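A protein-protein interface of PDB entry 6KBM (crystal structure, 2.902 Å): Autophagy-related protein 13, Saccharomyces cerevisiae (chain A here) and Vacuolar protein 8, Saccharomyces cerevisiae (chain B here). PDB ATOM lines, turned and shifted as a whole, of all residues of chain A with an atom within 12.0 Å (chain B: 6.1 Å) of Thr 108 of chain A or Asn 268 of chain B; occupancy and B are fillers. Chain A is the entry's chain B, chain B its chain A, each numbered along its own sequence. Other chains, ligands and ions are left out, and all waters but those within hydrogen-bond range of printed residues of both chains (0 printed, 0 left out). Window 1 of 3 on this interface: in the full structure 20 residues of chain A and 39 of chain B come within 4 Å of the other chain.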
ATOM      1  N   PRO A 101     -16.835  -1.839 -31.497  1.00  0.00           N
ATOM      2  CA  PRO A 101     -16.023  -2.953 -30.991  1.00  0.00           C
ATOM      3  C   PRO A 101     -14.655  -2.531 -30.462  1.00  0.00           C
ATOM      4  O   PRO A 101     -14.118  -3.185 -29.569  1.00  0.00           O
ATOM      5  CB  PRO A 101     -15.870  -3.852 -32.219  1.00  0.00           C
ATOM      6  CG  PRO A 101     -17.096  -3.598 -33.011  1.00  0.00           C
ATOM      7  CD  PRO A 101     -17.425  -2.145 -32.811  1.00  0.00           C
ATOM      8  N   TYR A 102     -14.100  -1.453 -31.004  1.00  0.00           N
ATOM      9  CA  TYR A 102     -12.799  -0.978 -30.558  1.00  0.00           C
ATOM     10  C   TYR A 102     -12.927   0.317 -29.772  1.00  0.00           C
ATOM     11  O   TYR A 102     -11.946   1.035 -29.572  1.00  0.00           O
ATOM     12  CB  TYR A 102     -11.861  -0.795 -31.752  1.00  0.00           C
ATOM     13  CG  TYR A 102     -11.582  -2.093 -32.472  1.00  0.00           C
ATOM     14  CD1 TYR A 102     -10.712  -3.033 -31.935  1.00  0.00           C
ATOM     15  CD2 TYR A 102     -12.206  -2.390 -33.675  1.00  0.00           C
ATOM     16  CE1 TYR A 102     -10.462  -4.224 -32.584  1.00  0.00           C
ATOM     17  CE2 TYR A 102     -11.961  -3.580 -34.331  1.00  0.00           C
ATOM     18  CZ  TYR A 102     -11.090  -4.493 -33.781  1.00  0.00           C
ATOM     19  OH  TYR A 102     -10.844  -5.679 -34.432  1.00  0.00           O
ATOM     20  N   TYR A 104     -12.941   1.312 -26.582  1.00  0.00           N
ATOM     21  CA  TYR A 104     -12.586   1.095 -25.189  1.00  0.00           C
ATOM     22  C   TYR A 104     -11.155   1.575 -25.016  1.00  0.00           C
ATOM     23  O   TYR A 104     -10.516   1.967 -25.989  1.00  0.00           O
ATOM     24  CB  TYR A 104     -12.732  -0.378 -24.794  1.00  0.00           C
ATOM     25  CG  TYR A 104     -11.829  -1.329 -25.553  1.00  0.00           C
ATOM     26  CD1 TYR A 104     -10.549  -1.617 -25.097  1.00  0.00           C
ATOM     27  CD2 TYR A 104     -12.260  -1.945 -26.720  1.00  0.00           C
ATOM     28  CE1 TYR A 104      -9.723  -2.485 -25.783  1.00  0.00           C
ATOM     29  CE2 TYR A 104     -11.440  -2.816 -27.413  1.00  0.00           C
ATOM     30  CZ  TYR A 104     -10.172  -3.081 -26.939  1.00  0.00           C
ATOM     31  OH  TYR A 104      -9.347  -3.947 -27.622  1.00  0.00           O
ATOM     32  N   SER A 105     -10.648   1.558 -23.791  1.00  0.00           N
ATOM     33  CA  SER A 105      -9.262   1.950 -23.579  1.00  0.00           C
ATOM     34  C   SER A 105      -8.356   0.807 -24.017  1.00  0.00           C
ATOM     35  O   SER A 105      -8.150  -0.155 -23.277  1.00  0.00           O
ATOM     36  CB  SER A 105      -9.007   2.321 -22.120  1.00  0.00           C
ATOM     37  OG  SER A 105      -7.709   2.868 -21.962  1.00  0.00           O
ATOM     38  N   GLN A 106      -7.828   0.915 -25.231  1.00  0.00           N
ATOM     39  CA  GLN A 106      -7.037  -0.157 -25.822  1.00  0.00           C
ATOM     40  C   GLN A 106      -5.700  -0.327 -25.112  1.00  0.00           C
ATOM     41  O   GLN A 106      -5.083   0.658 -24.704  1.00  0.00           O
ATOM     42  CB  GLN A 106      -6.819   0.112 -27.311  1.00  0.00           C
ATOM     43  CG  GLN A 106      -8.110   0.198 -28.104  1.00  0.00           C
ATOM     44  CD  GLN A 106      -7.873   0.170 -29.597  1.00  0.00           C
ATOM     45  OE1 GLN A 106      -7.370  -0.816 -30.137  1.00  0.00           O
ATOM     46  NE2 GLN A 106      -8.232   1.253 -30.275  1.00  0.00           N
ATOM     47  N   PRO A 107      -5.251  -1.586 -24.960  1.00  0.00           N
ATOM     48  CA  PRO A 107      -4.004  -1.894 -24.251  1.00  0.00           C
ATOM     49  C   PRO A 107      -2.797  -1.263 -24.923  1.00  0.00           C
ATOM     50  O   PRO A 107      -2.750  -1.184 -26.151  1.00  0.00           O
ATOM     51  CB  PRO A 107      -3.913  -3.424 -24.324  1.00  0.00           C
ATOM     52  CG  PRO A 107      -5.252  -3.891 -24.720  1.00  0.00           C
ATOM     53  CD  PRO A 107      -5.880  -2.796 -25.514  1.00  0.00           C
ATOM     54  N   THR A 108      -1.832  -0.820 -24.128  1.00  0.00           N
ATOM     55  CA  THR A 108      -0.617  -0.247 -24.682  1.00  0.00           C
ATOM     56  C   THR A 108       0.620  -0.859 -24.043  1.00  0.00           C
ATOM     57  O   THR A 108       0.558  -1.430 -22.954  1.00  0.00           O
ATOM     58  CB  THR A 108      -0.571   1.280 -24.501  1.00  0.00           C
ATOM     59  OG1 THR A 108       0.524   1.817 -25.254  1.00  0.00           O
ATOM     60  CG2 THR A 108      -0.393   1.640 -23.035  1.00  0.00           C
ATOM     61  N   THR A 109       1.745  -0.739 -24.738  1.00  0.00           N
ATOM     62  CA  THR A 109       3.021  -1.189 -24.209  1.00  0.00           C
ATOM     63  C   THR A 109       3.677  -0.065 -23.420  1.00  0.00           C
ATOM     64  O   THR A 109       3.866   1.035 -23.939  1.00  0.00           O
ATOM     65  CB  THR A 109       3.967  -1.647 -25.328  1.00  0.00           C
ATOM     66  OG1 THR A 109       3.365  -2.729 -26.051  1.00  0.00           O
ATOM     67  CG2 THR A 109       5.291  -2.104 -24.744  1.00  0.00           C
ATOM     68  N   ALA A 110       4.009  -0.341 -22.163  1.00  0.00           N
ATOM     69  CA  ALA A 110       4.667   0.647 -21.317  1.00  0.00           C
ATOM     70  C   ALA A 110       6.017   1.037 -21.906  1.00  0.00           C
ATOM     71  O   ALA A 110       6.780   0.176 -22.345  1.00  0.00           O
ATOM     72  CB  ALA A 110       4.834   0.112 -19.906  1.00  0.00           C
ATOM     73  N   PRO A 111       6.312   2.343 -21.922  1.00  0.00           N
ATOM     74  CA  PRO A 111       7.523   2.866 -22.562  1.00  0.00           C
ATOM     75  C   PRO A 111       8.792   2.671 -21.738  1.00  0.00           C
ATOM     76  O   PRO A 111       9.878   2.964 -22.236  1.00  0.00           O
ATOM     77  CB  PRO A 111       7.210   4.354 -22.716  1.00  0.00           C
ATOM     78  CG  PRO A 111       6.324   4.655 -21.558  1.00  0.00           C
ATOM     79  CD  PRO A 111       5.478   3.422 -21.362  1.00  0.00           C
ATOM     80  N   PHE A 112       8.662   2.188 -20.505  1.00  0.00           N
ATOM     81  CA  PHE A 112       9.822   2.040 -19.629  1.00  0.00           C
ATOM     82  C   PHE A 112      10.827   1.037 -20.177  1.00  0.00           C
ATOM     83  O   PHE A 112      10.458  -0.045 -20.635  1.00  0.00           O
ATOM     84  CB  PHE A 112       9.398   1.615 -18.220  1.00  0.00           C
ATOM     85  CG  PHE A 112      10.553   1.447 -17.268  1.00  0.00           C
ATOM     86  CD1 PHE A 112      11.077   2.537 -16.593  1.00  0.00           C
ATOM     87  CD2 PHE A 112      11.120   0.201 -17.053  1.00  0.00           C
ATOM     88  CE1 PHE A 112      12.141   2.387 -15.720  1.00  0.00           C
ATOM     89  CE2 PHE A 112      12.185   0.046 -16.183  1.00  0.00           C
ATOM     90  CZ  PHE A 112      12.693   1.140 -15.515  1.00  0.00           C
ATOM     91  N   LEU B 223       4.697  -7.927 -17.309  1.00  0.00           N
ATOM     92  CA  LEU B 223       3.394  -8.570 -17.433  1.00  0.00           C
ATOM     93  C   LEU B 223       2.377  -7.625 -18.071  1.00  0.00           C
ATOM     94  O   LEU B 223       1.564  -8.040 -18.901  1.00  0.00           O
ATOM     95  CB  LEU B 223       2.901  -9.048 -16.066  1.00  0.00           C
ATOM     96  CG  LEU B 223       3.619 -10.278 -15.504  1.00  0.00           C
ATOM     97  CD1 LEU B 223       2.945 -10.761 -14.236  1.00  0.00           C
ATOM     98  CD2 LEU B 223       3.673 -11.391 -16.539  1.00  0.00           C
ATOM     99  N   SER B 224       2.436  -6.354 -17.681  1.00  0.00           N
ATOM    100  CA  SER B 224       1.584  -5.326 -18.269  1.00  0.00           C
ATOM    101  C   SER B 224       1.795  -5.256 -19.776  1.00  0.00           C
ATOM    102  O   SER B 224       0.846  -5.077 -20.537  1.00  0.00           O
ATOM    103  CB  SER B 224       1.869  -3.962 -17.637  1.00  0.00           C
ATOM    104  OG  SER B 224       1.107  -2.939 -18.256  1.00  0.00           O
ATOM    105  N   ASN B 225       3.046  -5.404 -20.196  1.00  0.00           N
ATOM    106  CA  ASN B 225       3.386  -5.380 -21.610  1.00  0.00           C
ATOM    107  C   ASN B 225       2.948  -6.644 -22.335  1.00  0.00           C
ATOM    108  O   ASN B 225       2.606  -6.601 -23.514  1.00  0.00           O
ATOM    109  CB  ASN B 225       4.889  -5.174 -21.790  1.00  0.00           C
ATOM    110  CG  ASN B 225       5.321  -3.762 -21.467  1.00  0.00           C
ATOM    111  OD1 ASN B 225       4.496  -2.850 -21.404  1.00  0.00           O
ATOM    112  ND2 ASN B 225       6.619  -3.570 -21.265  1.00  0.00           N
ATOM    113  N   ALA B 227       0.290  -8.418 -21.501  1.00  0.00           N
ATOM    114  CA  ALA B 227      -1.172  -8.394 -21.551  1.00  0.00           C
ATOM    115  C   ALA B 227      -1.726  -7.646 -22.768  1.00  0.00           C
ATOM    116  O   ALA B 227      -2.930  -7.668 -23.017  1.00  0.00           O
ATOM    117  CB  ALA B 227      -1.724  -7.785 -20.272  1.00  0.00           C
ATOM    118  N   VAL B 228      -0.851  -6.985 -23.517  1.00  0.00           N
ATOM    119  CA  VAL B 228      -1.258  -6.250 -24.710  1.00  0.00           C
ATOM    120  C   VAL B 228      -1.833  -7.180 -25.784  1.00  0.00           C
ATOM    121  O   VAL B 228      -2.775  -6.819 -26.489  1.00  0.00           O
ATOM    122  CB  VAL B 228      -0.074  -5.446 -25.294  1.00  0.00           C
ATOM    123  CG1 VAL B 228      -0.473  -4.744 -26.580  1.00  0.00           C
ATOM    124  CG2 VAL B 228       0.423  -4.432 -24.278  1.00  0.00           C
ATOM    125  N   ARG B 233      -3.357 -12.978 -23.383  1.00  0.00           N
ATOM    126  CA  ARG B 233      -4.354 -12.797 -22.329  1.00  0.00           C
ATOM    127  C   ARG B 233      -5.121 -14.084 -22.053  1.00  0.00           C
ATOM    128  O   ARG B 233      -5.272 -14.488 -20.897  1.00  0.00           O
ATOM    129  CB  ARG B 233      -5.334 -11.678 -22.690  1.00  0.00           C
ATOM    130  CG  ARG B 233      -4.710 -10.296 -22.751  1.00  0.00           C
ATOM    131  CD  ARG B 233      -5.758  -9.203 -22.596  1.00  0.00           C
ATOM    132  NE  ARG B 233      -6.545  -9.006 -23.810  1.00  0.00           N
ATOM    133  CZ  ARG B 233      -6.205  -8.176 -24.791  1.00  0.00           C
ATOM    134  NH1 ARG B 233      -5.087  -7.467 -24.700  1.00  0.00           N
ATOM    135  NH2 ARG B 233      -6.979  -8.055 -25.862  1.00  0.00           N
ATOM    136  N   THR B 263      -2.212  -0.990 -12.307  1.00  0.00           N
ATOM    137  CA  THR B 263      -3.538  -0.548 -12.718  1.00  0.00           C
ATOM    138  C   THR B 263      -3.671  -0.617 -14.238  1.00  0.00           C
ATOM    139  O   THR B 263      -4.696  -1.062 -14.766  1.00  0.00           O
ATOM    140  CB  THR B 263      -3.825   0.880 -12.234  1.00  0.00           C
ATOM    141  OG1 THR B 263      -3.484   0.989 -10.846  1.00  0.00           O
ATOM    142  CG2 THR B 263      -5.293   1.219 -12.424  1.00  0.00           C
ATOM    143  N   LEU B 264      -2.625  -0.188 -14.936  1.00  0.00           N
ATOM    144  CA  LEU B 264      -2.605  -0.245 -16.396  1.00  0.00           C
ATOM    145  C   LEU B 264      -2.616  -1.686 -16.910  1.00  0.00           C
ATOM    146  O   LEU B 264      -3.262  -1.991 -17.916  1.00  0.00           O
ATOM    147  CB  LEU B 264      -1.384   0.497 -16.938  1.00  0.00           C
ATOM    148  CG  LEU B 264      -1.418   2.011 -16.727  1.00  0.00           C
ATOM    149  CD1 LEU B 264      -0.020   2.603 -16.778  1.00  0.00           C
ATOM    150  CD2 LEU B 264      -2.316   2.660 -17.766  1.00  0.00           C
ATOM    151  N   ALA B 265      -1.897  -2.563 -16.218  1.00  0.00           N
ATOM    152  CA  ALA B 265      -1.909  -3.987 -16.532  1.00  0.00           C
ATOM    153  C   ALA B 265      -3.325  -4.521 -16.397  1.00  0.00           C
ATOM    154  O   ALA B 265      -3.788  -5.319 -17.215  1.00  0.00           O
ATOM    155  CB  ALA B 265      -0.962  -4.748 -15.620  1.00  0.00           C
ATOM    156  N   LEU B 266      -4.010  -4.063 -15.356  1.00  0.00           N
ATOM    157  CA  LEU B 266      -5.390  -4.454 -15.120  1.00  0.00           C
ATOM    158  C   LEU B 266      -6.322  -3.903 -16.191  1.00  0.00           C
ATOM    159  O   LEU B 266      -7.354  -4.496 -16.477  1.00  0.00           O
ATOM    160  CB  LEU B 266      -5.844  -3.996 -13.736  1.00  0.00           C
ATOM    161  CG  LEU B 266      -5.322  -4.861 -12.589  1.00  0.00           C
ATOM    162  CD1 LEU B 266      -5.793  -4.327 -11.247  1.00  0.00           C
ATOM    163  CD2 LEU B 266      -5.762  -6.305 -12.780  1.00  0.00           C
ATOM    164  N   ARG B 267      -5.960  -2.768 -16.782  1.00  0.00           N
ATOM    165  CA  ARG B 267      -6.720  -2.238 -17.910  1.00  0.00           C
ATOM    166  C   ARG B 267      -6.556  -3.144 -19.131  1.00  0.00           C
ATOM    167  O   ARG B 267      -7.544  -3.633 -19.715  1.00  0.00           O
ATOM    168  CB  ARG B 267      -6.270  -0.818 -18.244  1.00  0.00           C
ATOM    169  CG  ARG B 267      -7.071  -0.175 -19.360  1.00  0.00           C
ATOM    170  CD  ARG B 267      -6.222   0.781 -20.173  1.00  0.00           C
ATOM    171  NE  ARG B 267      -4.904   0.230 -20.467  1.00  0.00           N
ATOM    172  CZ  ARG B 267      -3.864   0.960 -20.852  1.00  0.00           C
ATOM    173  NH1 ARG B 267      -3.991   2.271 -21.000  1.00  0.00           N
ATOM    174  NH2 ARG B 267      -2.699   0.378 -21.097  1.00  0.00           N
ATOM    175  N   ASN B 268      -5.296  -3.353 -19.507  1.00  0.00           N
ATOM    176  CA  ASN B 268      -4.933  -4.249 -20.600  1.00  0.00           C
ATOM    177  C   ASN B 268      -5.656  -5.583 -20.492  1.00  0.00           C
ATOM    178  O   ASN B 268      -6.187  -6.092 -21.478  1.00  0.00           O
ATOM    179  CB  ASN B 268      -3.421  -4.478 -20.620  1.00  0.00           C
ATOM    180  CG  ASN B 268      -2.644  -3.210 -20.901  1.00  0.00           C
ATOM    181  OD1 ASN B 268      -3.211  -2.119 -20.953  1.00  0.00           O
ATOM    182  ND2 ASN B 268      -1.336  -3.346 -21.075  1.00  0.00           N
ATOM    183  N   LEU B 269      -5.681  -6.140 -19.285  1.00  0.00           N
ATOM    184  CA  LEU B 269      -6.421  -7.369 -19.039  1.00  0.00           C
ATOM    185  C   LEU B 269      -7.919  -7.141 -19.189  1.00  0.00           C
ATOM    186  O   LEU B 269      -8.631  -7.985 -19.732  1.00  0.00           O
ATOM    187  CB  LEU B 269      -6.113  -7.918 -17.646  1.00  0.00           C
ATOM    188  CG  LEU B 269      -4.704  -8.465 -17.415  1.00  0.00           C
ATOM    189  CD1 LEU B 269      -4.553  -8.936 -15.980  1.00  0.00           C
ATOM    190  CD2 LEU B 269      -4.401  -9.594 -18.386  1.00  0.00           C
ATOM    191  N   ALA B 270      -8.390  -5.988 -18.721  1.00  0.00           N
ATOM    192  CA  ALA B 270      -9.817  -5.667 -18.740  1.00  0.00           C
ATOM    193  C   ALA B 270     -10.342  -5.476 -20.157  1.00  0.00           C
ATOM    194  O   ALA B 270     -11.542  -5.289 -20.358  1.00  0.00           O
ATOM    195  CB  ALA B 270     -10.094  -4.424 -17.909  1.00  0.00           C
ATOM    196  N   SER B 271      -9.446  -5.506 -21.137  1.00  0.00           N
ATOM    197  CA  SER B 271      -9.873  -5.540 -22.537  1.00  0.00           C
ATOM    198  C   SER B 271     -10.794  -6.728 -22.851  1.00  0.00           C
ATOM    199  O   SER B 271     -11.632  -6.647 -23.750  1.00  0.00           O
ATOM    200  CB  SER B 271      -8.659  -5.579 -23.461  1.00  0.00           C
ATOM    201  OG  SER B 271      -7.892  -4.401 -23.317  1.00  0.00           O
ATOM    202  N   ASP B 272     -10.632  -7.826 -22.115  1.00  0.00           N
ATOM    203  CA  ASP B 272     -11.446  -9.022 -22.328  1.00  0.00           C
ATOM    204  C   ASP B 272     -12.476  -9.207 -21.214  1.00  0.00           C
ATOM    205  O   ASP B 272     -12.248  -8.800 -20.077  1.00  0.00           O
ATOM    206  CB  ASP B 272     -10.556 -10.262 -22.431  1.00  0.00           C
ATOM    207  CG  ASP B 272      -9.611 -10.204 -23.618  1.00  0.00           C
ATOM    208  OD1 ASP B 272      -9.922  -9.489 -24.596  1.00  0.00           O
ATOM    209  OD2 ASP B 272      -8.558 -10.874 -23.572  1.00  0.00           O
ATOM    210  N   ASN B 309     -12.780   0.329 -19.060  1.00  0.00           N
ATOM    211  CA  ASN B 309     -12.768  -1.010 -19.639  1.00  0.00           C
ATOM    212  C   ASN B 309     -13.612  -2.010 -18.847  1.00  0.00           C
ATOM    213  O   ASN B 309     -14.288  -2.855 -19.433  1.00  0.00           O
ATOM    214  CB  ASN B 309     -11.333  -1.524 -19.765  1.00  0.00           C
ATOM    215  CG  ASN B 309     -10.626  -0.974 -20.990  1.00  0.00           C
ATOM    216  OD1 ASN B 309     -11.172  -0.142 -21.716  1.00  0.00           O
ATOM    217  ND2 ASN B 309      -9.408  -1.446 -21.231  1.00  0.00           N
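The backbone NH (N) of Ala 110 of chain A lies within hydrogen-bond range of the side-chain amide oxygen (OD1) of Asn 225 of chain B (2.7 Å).
The side-chain amide nitrogen of Asn 268 of chain B is in hydrogen-bond range of the backbone carbonyl oxygen of Thr 108 of chain A (3.3 Å).
ND2 of Asn 309 of chain B sits at hydrogen-bond distance from O of Ser 105 of chain A (2.7 Å).
NH2 of Arg 267 of chain B sits close to N of Thr 108 of chain A (3.4 Å).
The backbone carbonyl oxygen (O) of Ser 224 of chain B sits at hydrogen-bond distance from the side-chain amide nitrogen (ND2) of Asn 268 of chain B, at 2.8 Å.
The guanidinium group (NH1) of Arg 233 of chain B sits at hydrogen-bond distance from the backbone carbonyl oxygen (O) of Val 228 of chain B, 3.0 Å away.
OD2 of Asp 272 of chain B is in salt-bridge range of NE of Arg 233 of chain B, at 2.8 Å.
O of Leu 264 of chain B lies close to OD1 of Asn 268 of chain B, 3.0 Å away.
The guanidinium group of Arg 267 of chain B lies within hydrogen-bond range of the side-chain amide oxygen of Asn 268 of chain B, 2.6 Å away.
The backbone carbonyl oxygen of Arg 267 of chain B lies within hydrogen-bond range of the side-chain amide nitrogen of Asn 309 of chain B (3.2 Å).
Among the printed residues, pairs that only touch across the chains: Tyr 104 of chain A with Ser 271 of chain B (3.6 Å), Tyr 104 of chain A with Asn 309 of chain B (3.5 Å), Ser 105 of chain A with Arg 267 of chain B (3.1 Å), Pro 107 of chain A with Val 228 of chain B (3.9 Å), Pro 107 of chain A with Arg 233 of chain B (3.6 Å), Pro 107 of chain A with Asn 268 of chain B (3.4 Å), Pro 107 of chain A with Ser 271 of chain B (3.0 Å), Thr 108 of chain A with Val 228 of chain B (3.3 Å), Thr 109 of chain A with Asn 225 of chain B (3.5 Å) and Thr 109 of chain A with Val 228 of chain B (3.8 Å).
Pro 101 of chain A touches none of the printed residues of chain B.
Printed residues of chain B within 4 Å of Tyr 104 of chain A: Ser 271 and Asn 309.
Printed residues of chain B within 4 Å of Ser 105 of chain A: Arg 267 and Asn 309.
Of the printed residues of chain B, Pro 107 of chain A touches Val 228, Arg 233, Asn 268 and Ser 271.
Of the printed residues of chain B, Thr 108 of chain A touches Val 228, Arg 267 and Asn 268.
Printed residues of chain B within 4 Å of Thr 109 of chain A: Asn 225 and Val 228.
Printed residues of chain B within 4 Å of Ala 110 of chain A: Asn 225.
No residue of chain A comes within 4 Å of Ser 224 of chain B.
Asn 225 of chain B touches just these residues of chain A: Thr 109 (3.5 Å) and Ala 110 (2.7 Å).
No residue of chain A comes within 4 Å of Ala 227 of chain B.
Of the printed residues of chain A, Val 228 of chain B touches Pro 107, Thr 108 and Thr 109.
No residue of chain A comes within 4 Å of Leu 264 of chain B.
No residue of chain A comes within 4 Å of Ala 265 of chain B.
Asn 268 of chain B touches just these residues of chain A: Pro 107 (3.4 Å) and Thr 108 (3.3 Å).
No residue of chain A comes within 4 Å of Leu 269 of chain B.
No residue of chain A comes within 4 Å of Ala 270 of chain B.
Of chain A, only Tyr 104 and Pro 107 come within 4 Å of Ser 271 of chain B.
The nearest residue of chain B that does not touch Thr 108 of chain A is Ser 224 of chain B (4.4 Å).
The nearest residue of chain A that does not touch Asn 268 of chain B is Gln 106 of chain A (5.0 Å).
Hydrophobic or aromatic side chains of chain B within 4 Å of the printed part of chain A: Val 228.
Of the 11 printed residues of chain A, 6 touch a printed residue of chain B.
Along chain A the printed residues that touch a printed residue of chain B span positions 104 to 110.
Among the printed residues, no Asp or Glu carboxylate lies within 4 Å of a Lys or Arg side-chain nitrogen of the other chain.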
